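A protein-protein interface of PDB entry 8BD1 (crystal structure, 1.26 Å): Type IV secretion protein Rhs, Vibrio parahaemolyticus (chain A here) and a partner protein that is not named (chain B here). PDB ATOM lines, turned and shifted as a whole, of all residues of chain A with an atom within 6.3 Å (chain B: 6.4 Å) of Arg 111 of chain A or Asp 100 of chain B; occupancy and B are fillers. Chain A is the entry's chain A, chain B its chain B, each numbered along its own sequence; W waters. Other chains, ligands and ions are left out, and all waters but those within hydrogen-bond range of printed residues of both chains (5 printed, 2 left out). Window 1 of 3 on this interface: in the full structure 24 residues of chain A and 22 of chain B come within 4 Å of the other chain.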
ATOM      1  N   ARG A  12     -27.568  40.697   8.748  1.00  0.00           N
ATOM      2  CA  ARG A  12     -26.705  40.213   9.816  1.00  0.00           C
ATOM      3  C   ARG A  12     -25.261  40.213   9.339  1.00  0.00           C
ATOM      4  O   ARG A  12     -24.971  39.817   8.205  1.00  0.00           O
ATOM      5  CB  ARG A  12     -27.102  38.790  10.219  1.00  0.00           C
ATOM      6  CG  ARG A  12     -28.544  38.672  10.676  1.00  0.00           C
ATOM      7  CD  ARG A  12     -28.866  37.268  11.212  1.00  0.00           C
ATOM      8  NE  ARG A  12     -28.015  36.879  12.336  1.00  0.00           N
ATOM      9  CZ  ARG A  12     -28.174  37.311  13.580  1.00  0.00           C
ATOM     10  NH1 ARG A  12     -29.153  38.146  13.902  1.00  0.00           N
ATOM     11  NH2 ARG A  12     -27.314  36.920  14.514  1.00  0.00           N
ATOM     12  N   THR A  55     -33.427  24.892   0.291  1.00  0.00           N
ATOM     13  CA  THR A  55     -34.154  25.890   1.062  1.00  0.00           C
ATOM     14  C   THR A  55     -33.385  26.396   2.265  1.00  0.00           C
ATOM     15  O   THR A  55     -33.756  27.436   2.827  1.00  0.00           O
ATOM     16  CB  THR A  55     -35.483  25.314   1.564  1.00  0.00           C
ATOM     17  OG1 THR A  55     -35.197  24.291   2.519  1.00  0.00           O
ATOM     18  CG2 THR A  55     -36.289  24.721   0.415  1.00  0.00           C
ATOM     19  N   GLY A  56     -32.326  25.712   2.677  1.00  0.00           N
ATOM     20  CA  GLY A  56     -31.683  26.009   3.937  1.00  0.00           C
ATOM     21  C   GLY A  56     -32.203  25.184   5.097  1.00  0.00           C
ATOM     22  O   GLY A  56     -31.609  25.216   6.180  1.00  0.00           O
ATOM     23  N   ASP A  57     -33.284  24.442   4.901  1.00  0.00           N
ATOM     24  CA  ASP A  57     -33.775  23.473   5.878  1.00  0.00           C
ATOM     25  C   ASP A  57     -32.858  22.250   5.833  1.00  0.00           C
ATOM     26  O   ASP A  57     -32.850  21.514   4.844  1.00  0.00           O
ATOM     27  CB  ASP A  57     -35.206  23.138   5.464  1.00  0.00           C
ATOM     28  CG  ASP A  57     -35.861  22.056   6.308  1.00  0.00           C
ATOM     29  OD1 ASP A  57     -35.174  21.191   6.881  1.00  0.00           O
ATOM     30  OD2 ASP A  57     -37.107  22.045   6.363  1.00  0.00           O
ATOM     31  N   MET A  58     -32.053  22.033   6.880  1.00  0.00           N
ATOM     32  CA  MET A  58     -31.043  20.971   6.844  1.00  0.00           C
ATOM     33  C   MET A  58     -31.657  19.613   6.552  1.00  0.00           C
ATOM     34  O   MET A  58     -31.163  18.860   5.706  1.00  0.00           O
ATOM     35  CB  MET A  58     -30.277  20.877   8.169  1.00  0.00           C
ATOM     36  CG  MET A  58     -29.440  22.066   8.453  1.00  0.00           C
ATOM     37  SD  MET A  58     -27.981  22.225   7.400  1.00  0.00           S
ATOM     38  CE  MET A  58     -27.331  20.564   7.212  1.00  0.00           C
ATOM     39  N   ASP A  61     -32.740  19.388   2.993  1.00  0.00           N
ATOM     40  CA  ASP A  61     -31.709  19.561   1.974  1.00  0.00           C
ATOM     41  C   ASP A  61     -30.700  18.416   1.961  1.00  0.00           C
ATOM     42  O   ASP A  61     -30.207  18.045   0.889  1.00  0.00           O
ATOM     43  CB  ASP A  61     -30.974  20.884   2.196  1.00  0.00           C
ATOM     44  CG  ASP A  61     -31.794  22.114   1.811  1.00  0.00           C
ATOM     45  OD1 ASP A  61     -32.937  21.995   1.307  1.00  0.00           O
ATOM     46  OD2 ASP A  61     -31.263  23.207   2.043  1.00  0.00           O
ATOM     47  N   HIS A  83     -23.752  24.325   3.246  1.00  0.00           N
ATOM     48  CA  HIS A  83     -24.415  25.019   2.150  1.00  0.00           C
ATOM     49  C   HIS A  83     -23.452  26.069   1.608  1.00  0.00           C
ATOM     50  O   HIS A  83     -23.096  27.018   2.311  1.00  0.00           O
ATOM     51  CB  HIS A  83     -25.666  25.734   2.655  1.00  0.00           C
ATOM     52  CG  HIS A  83     -26.834  24.835   2.904  1.00  0.00           C
ATOM     53  ND1 HIS A  83     -26.939  24.022   4.016  1.00  0.00           N
ATOM     54  CD2 HIS A  83     -27.975  24.659   2.202  1.00  0.00           C
ATOM     55  CE1 HIS A  83     -28.095  23.386   3.983  1.00  0.00           C
ATOM     56  NE2 HIS A  83     -28.743  23.756   2.893  1.00  0.00           N
ATOM     57  N   HIS A  84     -23.034  25.911   0.353  1.00  0.00           N
ATOM     58  CA  HIS A  84     -22.228  26.943  -0.277  1.00  0.00           C
ATOM     59  C   HIS A  84     -23.059  28.209  -0.476  1.00  0.00           C
ATOM     60  O   HIS A  84     -24.283  28.156  -0.642  1.00  0.00           O
ATOM     61  CB  HIS A  84     -21.700  26.444  -1.619  1.00  0.00           C
ATOM     62  CG  HIS A  84     -20.628  27.305  -2.197  1.00  0.00           C
ATOM     63  ND1 HIS A  84     -20.897  28.403  -2.985  1.00  0.00           N
ATOM     64  CD2 HIS A  84     -19.283  27.249  -2.068  1.00  0.00           C
ATOM     65  CE1 HIS A  84     -19.758  28.977  -3.331  1.00  0.00           C
ATOM     66  NE2 HIS A  84     -18.767  28.291  -2.792  1.00  0.00           N
ATOM     67  N   GLY A 109     -23.097  30.689   6.055  1.00  0.00           N
ATOM     68  CA  GLY A 109     -23.144  29.924   4.827  1.00  0.00           C
ATOM     69  C   GLY A 109     -24.370  30.163   3.972  1.00  0.00           C
ATOM     70  O   GLY A 109     -25.111  31.140   4.153  1.00  0.00           O
ATOM     71  N   GLY A 110     -24.603  29.254   3.026  1.00  0.00           N
ATOM     72  CA  GLY A 110     -25.643  29.420   2.034  1.00  0.00           C
ATOM     73  C   GLY A 110     -27.061  29.378   2.566  1.00  0.00           C
ATOM     74  O   GLY A 110     -27.971  29.833   1.868  1.00  0.00           O
ATOM     75  N   ARG A 111     -27.288  28.830   3.770  1.00  0.00           N
ATOM     76  CA  ARG A 111     -28.640  28.905   4.317  1.00  0.00           C
ATOM     77  C   ARG A 111     -29.089  30.352   4.437  1.00  0.00           C
ATOM     78  O   ARG A 111     -30.239  30.683   4.111  1.00  0.00           O
ATOM     79  CB  ARG A 111     -28.714  28.229   5.687  1.00  0.00           C
ATOM     80  CG  ARG A 111     -28.451  26.722   5.639  1.00  0.00           C
ATOM     81  CD  ARG A 111     -28.354  26.103   7.022  1.00  0.00           C
ATOM     82  NE  ARG A 111     -29.605  26.194   7.760  1.00  0.00           N
ATOM     83  CZ  ARG A 111     -29.755  26.891   8.879  1.00  0.00           C
ATOM     84  NH1 ARG A 111     -28.763  27.604   9.390  1.00  0.00           N
ATOM     85  NH2 ARG A 111     -30.935  26.890   9.490  1.00  0.00           N
ATOM     86  N   SER A 112     -28.185  31.225   4.886  1.00  0.00           N
ATOM     87  CA  SER A 112     -28.507  32.642   5.001  1.00  0.00           C
ATOM     88  C   SER A 112     -28.735  33.253   3.625  1.00  0.00           C
ATOM     89  O   SER A 112     -29.676  34.032   3.432  1.00  0.00           O
ATOM     90  CB  SER A 112     -27.373  33.394   5.710  1.00  0.00           C
ATOM     91  OG  SER A 112     -26.174  33.330   4.960  1.00  0.00           O
ATOM     92  N   VAL A 113     -27.887  32.908   2.652  1.00  0.00           N
ATOM     93  CA  VAL A 113     -27.992  33.517   1.329  1.00  0.00           C
ATOM     94  C   VAL A 113     -29.297  33.124   0.655  1.00  0.00           C
ATOM     95  O   VAL A 113     -29.969  33.966   0.034  1.00  0.00           O
ATOM     96  CB  VAL A 113     -26.761  33.170   0.465  1.00  0.00           C
ATOM     97  CG1 VAL A 113     -26.900  33.761  -0.932  1.00  0.00           C
ATOM     98  CG2 VAL A 113     -25.492  33.648   1.127  1.00  0.00           C
ATOM     99  N   ILE A 114     -29.682  31.850   0.758  1.00  0.00           N
ATOM    100  CA  ILE A 114     -30.944  31.421   0.172  1.00  0.00           C
ATOM    101  C   ILE A 114     -32.089  32.251   0.734  1.00  0.00           C
ATOM    102  O   ILE A 114     -32.931  32.769  -0.007  1.00  0.00           O
ATOM    103  CB  ILE A 114     -31.167  29.918   0.401  1.00  0.00           C
ATOM    104  CG1 ILE A 114     -30.134  29.097  -0.386  1.00  0.00           C
ATOM    105  CG2 ILE A 114     -32.589  29.541   0.038  1.00  0.00           C
ATOM    106  CD1 ILE A 114     -29.973  27.669   0.092  1.00  0.00           C
ATOM    107  N   GLN A 115     -32.116  32.410   2.061  1.00  0.00           N
ATOM    108  CA  GLN A 115     -33.194  33.161   2.695  1.00  0.00           C
ATOM    109  C   GLN A 115     -33.114  34.654   2.373  1.00  0.00           C
ATOM    110  O   GLN A 115     -34.143  35.307   2.159  1.00  0.00           O
ATOM    111  CB  GLN A 115     -33.181  32.891   4.200  1.00  0.00           C
ATOM    112  CG  GLN A 115     -33.526  31.433   4.509  1.00  0.00           C
ATOM    113  CD  GLN A 115     -34.898  31.068   3.999  1.00  0.00           C
ATOM    114  OE1 GLN A 115     -35.849  31.832   4.170  1.00  0.00           O
ATOM    115  NE2 GLN A 115     -35.019  29.916   3.365  1.00  0.00           N
ATOM    116  N   HIS A 116     -31.908  35.208   2.318  1.00  0.00           N
ATOM    117  CA  HIS A 116     -31.736  36.590   1.889  1.00  0.00           C
ATOM    118  C   HIS A 116     -32.324  36.800   0.495  1.00  0.00           C
ATOM    119  O   HIS A 116     -33.022  37.793   0.228  1.00  0.00           O
ATOM    120  CB  HIS A 116     -30.239  36.901   1.904  1.00  0.00           C
ATOM    121  CG  HIS A 116     -29.888  38.232   1.327  1.00  0.00           C
ATOM    122  ND1 HIS A 116     -29.563  39.319   2.107  1.00  0.00           N
ATOM    123  CD2 HIS A 116     -29.786  38.643   0.043  1.00  0.00           C
ATOM    124  CE1 HIS A 116     -29.299  40.354   1.327  1.00  0.00           C
ATOM    125  NE2 HIS A 116     -29.425  39.967   0.071  1.00  0.00           N
ATOM    126  N   ILE B  40     -36.095  30.752  11.032  1.00  0.00           N
ATOM    127  CA  ILE B  40     -35.327  29.769  10.271  1.00  0.00           C
ATOM    128  C   ILE B  40     -36.257  29.047   9.315  1.00  0.00           C
ATOM    129  O   ILE B  40     -37.472  28.981   9.540  1.00  0.00           O
ATOM    130  CB  ILE B  40     -34.587  28.769  11.193  1.00  0.00           C
ATOM    131  CG1 ILE B  40     -35.562  27.839  11.928  1.00  0.00           C
ATOM    132  CG2 ILE B  40     -33.666  29.501  12.146  1.00  0.00           C
ATOM    133  CD1 ILE B  40     -34.859  26.704  12.666  1.00  0.00           C
ATOM    134  N   PRO B  41     -35.713  28.468   8.241  1.00  0.00           N
ATOM    135  CA  PRO B  41     -36.556  27.725   7.296  1.00  0.00           C
ATOM    136  C   PRO B  41     -36.830  26.290   7.708  1.00  0.00           C
ATOM    137  O   PRO B  41     -37.769  25.688   7.172  1.00  0.00           O
ATOM    138  CB  PRO B  41     -35.730  27.759   6.004  1.00  0.00           C
ATOM    139  CG  PRO B  41     -34.326  27.806   6.475  1.00  0.00           C
ATOM    140  CD  PRO B  41     -34.346  28.660   7.726  1.00  0.00           C
ATOM    141  N   ASP B  42     -36.048  25.718   8.626  1.00  0.00           N
ATOM    142  CA  ASP B  42     -36.160  24.298   8.945  1.00  0.00           C
ATOM    143  C   ASP B  42     -37.511  23.987   9.571  1.00  0.00           C
ATOM    144  O   ASP B  42     -37.987  24.716  10.441  1.00  0.00           O
ATOM    145  CB  ASP B  42     -35.074  23.895   9.947  1.00  0.00           C
ATOM    146  CG  ASP B  42     -33.679  24.336   9.539  1.00  0.00           C
ATOM    147  OD1 ASP B  42     -33.451  25.549   9.344  1.00  0.00           O
ATOM    148  OD2 ASP B  42     -32.788  23.463   9.491  1.00  0.00           O
ATOM    149  N   ILE B  45     -35.611  20.195  13.628  1.00  0.00           N
ATOM    150  CA  ILE B  45     -34.189  20.222  13.959  1.00  0.00           C
ATOM    151  C   ILE B  45     -33.789  18.835  14.432  1.00  0.00           C
ATOM    152  O   ILE B  45     -34.285  18.347  15.460  1.00  0.00           O
ATOM    153  CB  ILE B  45     -33.856  21.276  15.022  1.00  0.00           C
ATOM    154  CG1 ILE B  45     -34.284  22.665  14.539  1.00  0.00           C
ATOM    155  CG2 ILE B  45     -32.366  21.254  15.350  1.00  0.00           C
ATOM    156  CD1 ILE B  45     -33.642  23.082  13.231  1.00  0.00           C
ATOM    157  N   GLU B  81     -24.943  22.989  11.673  1.00  0.00           N
ATOM    158  CA  GLU B  81     -24.136  23.617  12.710  1.00  0.00           C
ATOM    159  C   GLU B  81     -24.959  24.208  13.842  1.00  0.00           C
ATOM    160  O   GLU B  81     -24.376  24.600  14.856  1.00  0.00           O
ATOM    161  CB  GLU B  81     -23.205  24.685  12.126  1.00  0.00           C
ATOM    162  CG  GLU B  81     -22.082  24.107  11.280  1.00  0.00           C
ATOM    163  CD  GLU B  81     -21.190  23.150  12.042  1.00  0.00           C
ATOM    164  OE1 GLU B  81     -21.113  23.248  13.283  1.00  0.00           O
ATOM    165  OE2 GLU B  81     -20.557  22.301  11.385  1.00  0.00           O
ATOM    166  N   ALA B  82     -26.281  24.269  13.715  1.00  0.00           N
ATOM    167  CA  ALA B  82     -27.070  24.814  14.810  1.00  0.00           C
ATOM    168  C   ALA B  82     -26.831  24.014  16.082  1.00  0.00           C
ATOM    169  O   ALA B  82     -26.609  22.801  16.051  1.00  0.00           O
ATOM    170  CB  ALA B  82     -28.554  24.764  14.466  1.00  0.00           C
ATOM    171  N   VAL B  83     -26.919  24.702  17.213  1.00  0.00           N
ATOM    172  CA  VAL B  83     -26.806  24.054  18.512  1.00  0.00           C
ATOM    173  C   VAL B  83     -28.016  24.403  19.364  1.00  0.00           C
ATOM    174  O   VAL B  83     -28.580  25.499  19.264  1.00  0.00           O
ATOM    175  CB  VAL B  83     -25.488  24.403  19.243  1.00  0.00           C
ATOM    176  CG1 VAL B  83     -24.330  23.654  18.608  1.00  0.00           C
ATOM    177  CG2 VAL B  83     -25.225  25.909  19.230  1.00  0.00           C
ATOM    178  N   TYR B  98     -32.437  27.864  20.544  1.00  0.00           N
ATOM    179  CA  TYR B  98     -31.776  27.475  19.308  1.00  0.00           C
ATOM    180  C   TYR B  98     -30.764  28.557  18.959  1.00  0.00           C
ATOM    181  O   TYR B  98     -31.032  29.747  19.141  1.00  0.00           O
ATOM    182  CB  TYR B  98     -32.827  27.391  18.196  1.00  0.00           C
ATOM    183  CG  TYR B  98     -32.296  27.146  16.793  1.00  0.00           C
ATOM    184  CD1 TYR B  98     -31.824  28.195  16.007  1.00  0.00           C
ATOM    185  CD2 TYR B  98     -32.299  25.873  16.257  1.00  0.00           C
ATOM    186  CE1 TYR B  98     -31.346  27.975  14.722  1.00  0.00           C
ATOM    187  CE2 TYR B  98     -31.829  25.640  14.980  1.00  0.00           C
ATOM    188  CZ  TYR B  98     -31.366  26.694  14.214  1.00  0.00           C
ATOM    189  OH  TYR B  98     -30.895  26.446  12.938  1.00  0.00           O
ATOM    190  N   PHE B  99     -29.604  28.159  18.456  1.00  0.00           N
ATOM    191  CA  PHE B  99     -28.633  29.123  17.955  1.00  0.00           C
ATOM    192  C   PHE B  99     -27.985  28.604  16.682  1.00  0.00           C
ATOM    193  O   PHE B  99     -27.614  27.433  16.610  1.00  0.00           O
ATOM    194  CB  PHE B  99     -27.521  29.418  18.980  1.00  0.00           C
ATOM    195  CG  PHE B  99     -26.456  30.314  18.438  1.00  0.00           C
ATOM    196  CD1 PHE B  99     -26.618  31.686  18.477  1.00  0.00           C
ATOM    197  CD2 PHE B  99     -25.308  29.794  17.852  1.00  0.00           C
ATOM    198  CE1 PHE B  99     -25.657  32.535  17.948  1.00  0.00           C
ATOM    199  CE2 PHE B  99     -24.344  30.631  17.325  1.00  0.00           C
ATOM    200  CZ  PHE B  99     -24.522  32.014  17.374  1.00  0.00           C
ATOM    201  N   ASP B 100     -27.815  29.484  15.690  1.00  0.00           N
ATOM    202  CA  ASP B 100     -26.915  29.183  14.583  1.00  0.00           C
ATOM    203  C   ASP B 100     -26.258  30.468  14.097  1.00  0.00           C
ATOM    204  O   ASP B 100     -26.664  31.581  14.453  1.00  0.00           O
ATOM    205  CB  ASP B 100     -27.562  28.303  13.483  1.00  0.00           C
ATOM    206  CG  ASP B 100     -28.516  29.059  12.573  1.00  0.00           C
ATOM    207  OD1 ASP B 100     -28.298  30.262  12.339  1.00  0.00           O
ATOM    208  OD2 ASP B 100     -29.465  28.435  12.047  1.00  0.00           O
ATOM    209  N   PHE B 101     -25.228  30.300  13.277  1.00  0.00           N
ATOM    210  CA  PHE B 101     -24.430  31.411  12.784  1.00  0.00           C
ATOM    211  C   PHE B 101     -24.996  32.058  11.529  1.00  0.00           C
ATOM    212  O   PHE B 101     -24.396  33.014  11.016  1.00  0.00           O
ATOM    213  CB  PHE B 101     -22.984  30.957  12.547  1.00  0.00           C
ATOM    214  CG  PHE B 101     -22.204  30.748  13.814  1.00  0.00           C
ATOM    215  CD1 PHE B 101     -21.931  31.815  14.651  1.00  0.00           C
ATOM    216  CD2 PHE B 101     -21.752  29.491  14.174  1.00  0.00           C
ATOM    217  CE1 PHE B 101     -21.224  31.635  15.825  1.00  0.00           C
ATOM    218  CE2 PHE B 101     -21.038  29.308  15.344  1.00  0.00           C
ATOM    219  CZ  PHE B 101     -20.776  30.383  16.168  1.00  0.00           C
ATOM    220  N   ASP B 102     -26.133  31.582  11.031  1.00  0.00           N
ATOM    221  CA  ASP B 102     -26.804  32.193   9.897  1.00  0.00           C
ATOM    222  C   ASP B 102     -27.926  33.130  10.318  1.00  0.00           C
ATOM    223  O   ASP B 102     -28.120  34.183   9.697  1.00  0.00           O
ATOM    224  CB  ASP B 102     -27.382  31.097   8.995  1.00  0.00           C
ATOM    225  CG  ASP B 102     -26.316  30.263   8.325  1.00  0.00           C
ATOM    226  OD1 ASP B 102     -25.366  30.863   7.788  1.00  0.00           O
ATOM    227  OD2 ASP B 102     -26.448  29.018   8.305  1.00  0.00           O
ATOM    228  N   PHE B 103     -28.655  32.773  11.373  1.00  0.00           N
ATOM    229  CA  PHE B 103     -29.865  33.465  11.778  1.00  0.00           C
ATOM    230  C   PHE B 103     -29.858  33.936  13.222  1.00  0.00           C
ATOM    231  O   PHE B 103     -30.696  34.779  13.573  1.00  0.00           O
ATOM    232  CB  PHE B 103     -31.085  32.571  11.528  1.00  0.00           C
ATOM    233  CG  PHE B 103     -31.191  32.096  10.100  1.00  0.00           C
ATOM    234  CD1 PHE B 103     -31.568  32.971   9.098  1.00  0.00           C
ATOM    235  CD2 PHE B 103     -30.887  30.784   9.753  1.00  0.00           C
ATOM    236  CE1 PHE B 103     -31.655  32.555   7.779  1.00  0.00           C
ATOM    237  CE2 PHE B 103     -30.964  30.364   8.417  1.00  0.00           C
ATOM    238  CZ  PHE B 103     -31.356  31.259   7.444  1.00  0.00           C
ATOM    239  N   GLY B 104     -28.958  33.444  14.063  1.00  0.00           N
ATOM    240  CA  GLY B 104     -28.846  33.922  15.430  1.00  0.00           C
ATOM    241  C   GLY B 104     -29.475  33.005  16.461  1.00  0.00           C
ATOM    242  O   GLY B 104     -29.642  31.800  16.266  1.00  0.00           O
ATOM    243  N   ALA B 105     -29.811  33.606  17.600  1.00  0.00           N
ATOM    244  CA  ALA B 105     -30.350  32.907  18.756  1.00  0.00           C
ATOM    245  C   ALA B 105     -31.853  33.109  18.828  1.00  0.00           C
ATOM    246  O   ALA B 105     -32.383  34.139  18.396  1.00  0.00           O
ATOM    247  CB  ALA B 105     -29.709  33.449  20.040  1.00  0.00           C
HETATM  248  O   HOH W   1     -33.229  20.794   9.741  1.00  0.00           O
HETATM  249  O   HOH W   2     -25.742  24.483   9.225  1.00  0.00           O
HETATM  250  O   HOH W   3     -30.592  24.041  11.322  1.00  0.00           O
HETATM  251  O   HOH W   4     -25.565  34.266  14.547  1.00  0.00           O
HETATM  252  O   HOH W   5     -25.435  35.598  12.170  1.00  0.00           O
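The side-chain carboxylate (OD2) of Asp 42 of chain B lies within hydrogen-bond range of the backbone NH (N) of Met 58 of chain A, 3.1 Å away.
N of Gly 109 of chain A sits at hydrogen-bond distance from OD1 of Asp 102 of chain B, at 2.9 Å.
NH2 of Arg 111 of chain A is in salt-bridge range of OD1 of Asp 42 of chain B, 2.9 Å away.
NH2 of Arg 111 of chain A is in hydrogen-bond range of OH of Tyr 98 of chain B, 3.5 Å away.
The guanidinium group (NH1) of Arg 111 of chain A is in salt-bridge range of the side-chain carboxylate (OD2) of Asp 100 of chain B.
The side-chain carboxylate (OD2) of Asp 102 of chain B lies within salt-bridge range of the guanidinium group (NH1) of Arg 111 of chain A, at 2.9 Å.
N of Thr 55 of chain A is in hydrogen-bond range of OD1 of Asp 61 of chain A (3.1 Å).
NE2 of Gln 115 of chain A sits at hydrogen-bond distance from O of Thr 55 of chain A (2.8 Å).
The backbone carbonyl oxygen (O) of Gly 109 of chain A sits at hydrogen-bond distance from the side-chain hydroxyl (OG) of Ser 112 of chain A (2.6 Å).
OH of Tyr 98 of chain B sits at hydrogen-bond distance from OD2 of Asp 100 of chain B, at 2.6 Å.
N of Asp 102 of chain B sits at hydrogen-bond distance from OD1 of Asp 100 of chain B (2.9 Å).
The backbone NH of Phe 103 of chain B is in hydrogen-bond range of the side-chain carboxylate of Asp 100 of chain B, 2.7 Å away.
Arg 12 of chain A touches Asp 102 of chain B.
Phe 103 of chain B touches Arg 12 of chain A.
Arg 12 of chain A touches Gly 104 of chain B (NH2 to CA, 3.5 Å).
Pro 41 of chain B touches Gly 56 of chain A.
Asp 57 of chain A touches Asp 42 of chain B (CG to CA, 3.5 Å).
Arg 111 of chain A touches Phe 103 of chain B.
Asp 102 of chain B touches Ser 112 of chain A.
Ser 112 of chain A touches Phe 103 of chain B (CA to CZ, 3.9997 Å).
CB of Pro 41 of chain B touches NE2 of Gln 115 of chain A, 3.5 Å away.
Phe 103 of chain B touches Gln 115 of chain A (CZ to CG, 3.7 Å).
Arg 111 of chain A touches five residues of chain B.
Of chain A, only Arg 111 comes within 4 Å of Asp 100 of chain B.
Of the printed residues of chain A, Phe 103 of chain B touches Arg 12, Arg 111, Ser 112 and Gln 115.
Printed residues of chain B within 4 Å of Ser 112 of chain A: Asp 102 (3.8 Å) and Phe 103 (3.9997 Å).
Printed residues of chain B within 4 Å of Gln 115 of chain A: Pro 41 (3.5 Å) and Phe 103 (3.7 Å).
Printed residues of chain A within 4 Å of Asp 102 of chain B: Arg 12, Gly 109, Arg 111 and Ser 112.
Printed residues of chain B within 4 Å of Gly 56 of chain A: Pro 41 (3.6 Å) and Asp 42 (3.7 Å).
Gly 110 of chain A touches none of the printed residues of chain B.
Ala 105 of chain B touches none of the printed residues of chain A.
The nearest residue of chain B that does not touch Arg 111 of chain A is Pro 41 of chain B (4.2 Å).
Of the 16 printed residues of chain A, 9 touch a printed residue of chain B.
Hydrophobic or aromatic side chains of chain A within 4 Å of the printed part of chain B: Met 58.
Of the 15 printed residues of chain B, 7 touch a printed residue of chain A.
Among the printed residues, 19 pairs touch across the chains.
Water W1 lies within hydrogen-bond range of OD2 of Asp 42 of chain B, N of Met 58 of chain A and OD1 of Asp 57 of chain A.
Water W5 bridges the guanidinium group (NE) of Arg 12 of chain A (2.9 Å) and the backbone carbonyl oxygen (O) of Phe 101 of chain B (3.0 Å).
Water W4 lies within hydrogen-bond range of the backbone carbonyl oxygen of Asp 100 of chain B (2.9 Å) and the guanidinium group of Arg 12 of chain A (3.2 Å).
Water W3 lies within hydrogen-bond range of the side-chain hydroxyl of Tyr 98 of chain B (2.9 Å), the side-chain carboxylate of Asp 42 of chain B (2.9 Å) and the guanidinium group of Arg 111 of chain A (3.4 Å).
Water W2 lies within hydrogen-bond range of N of Glu 81 of chain B (3.0 Å) and SD of Met 58 of chain A (3.7 Å).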
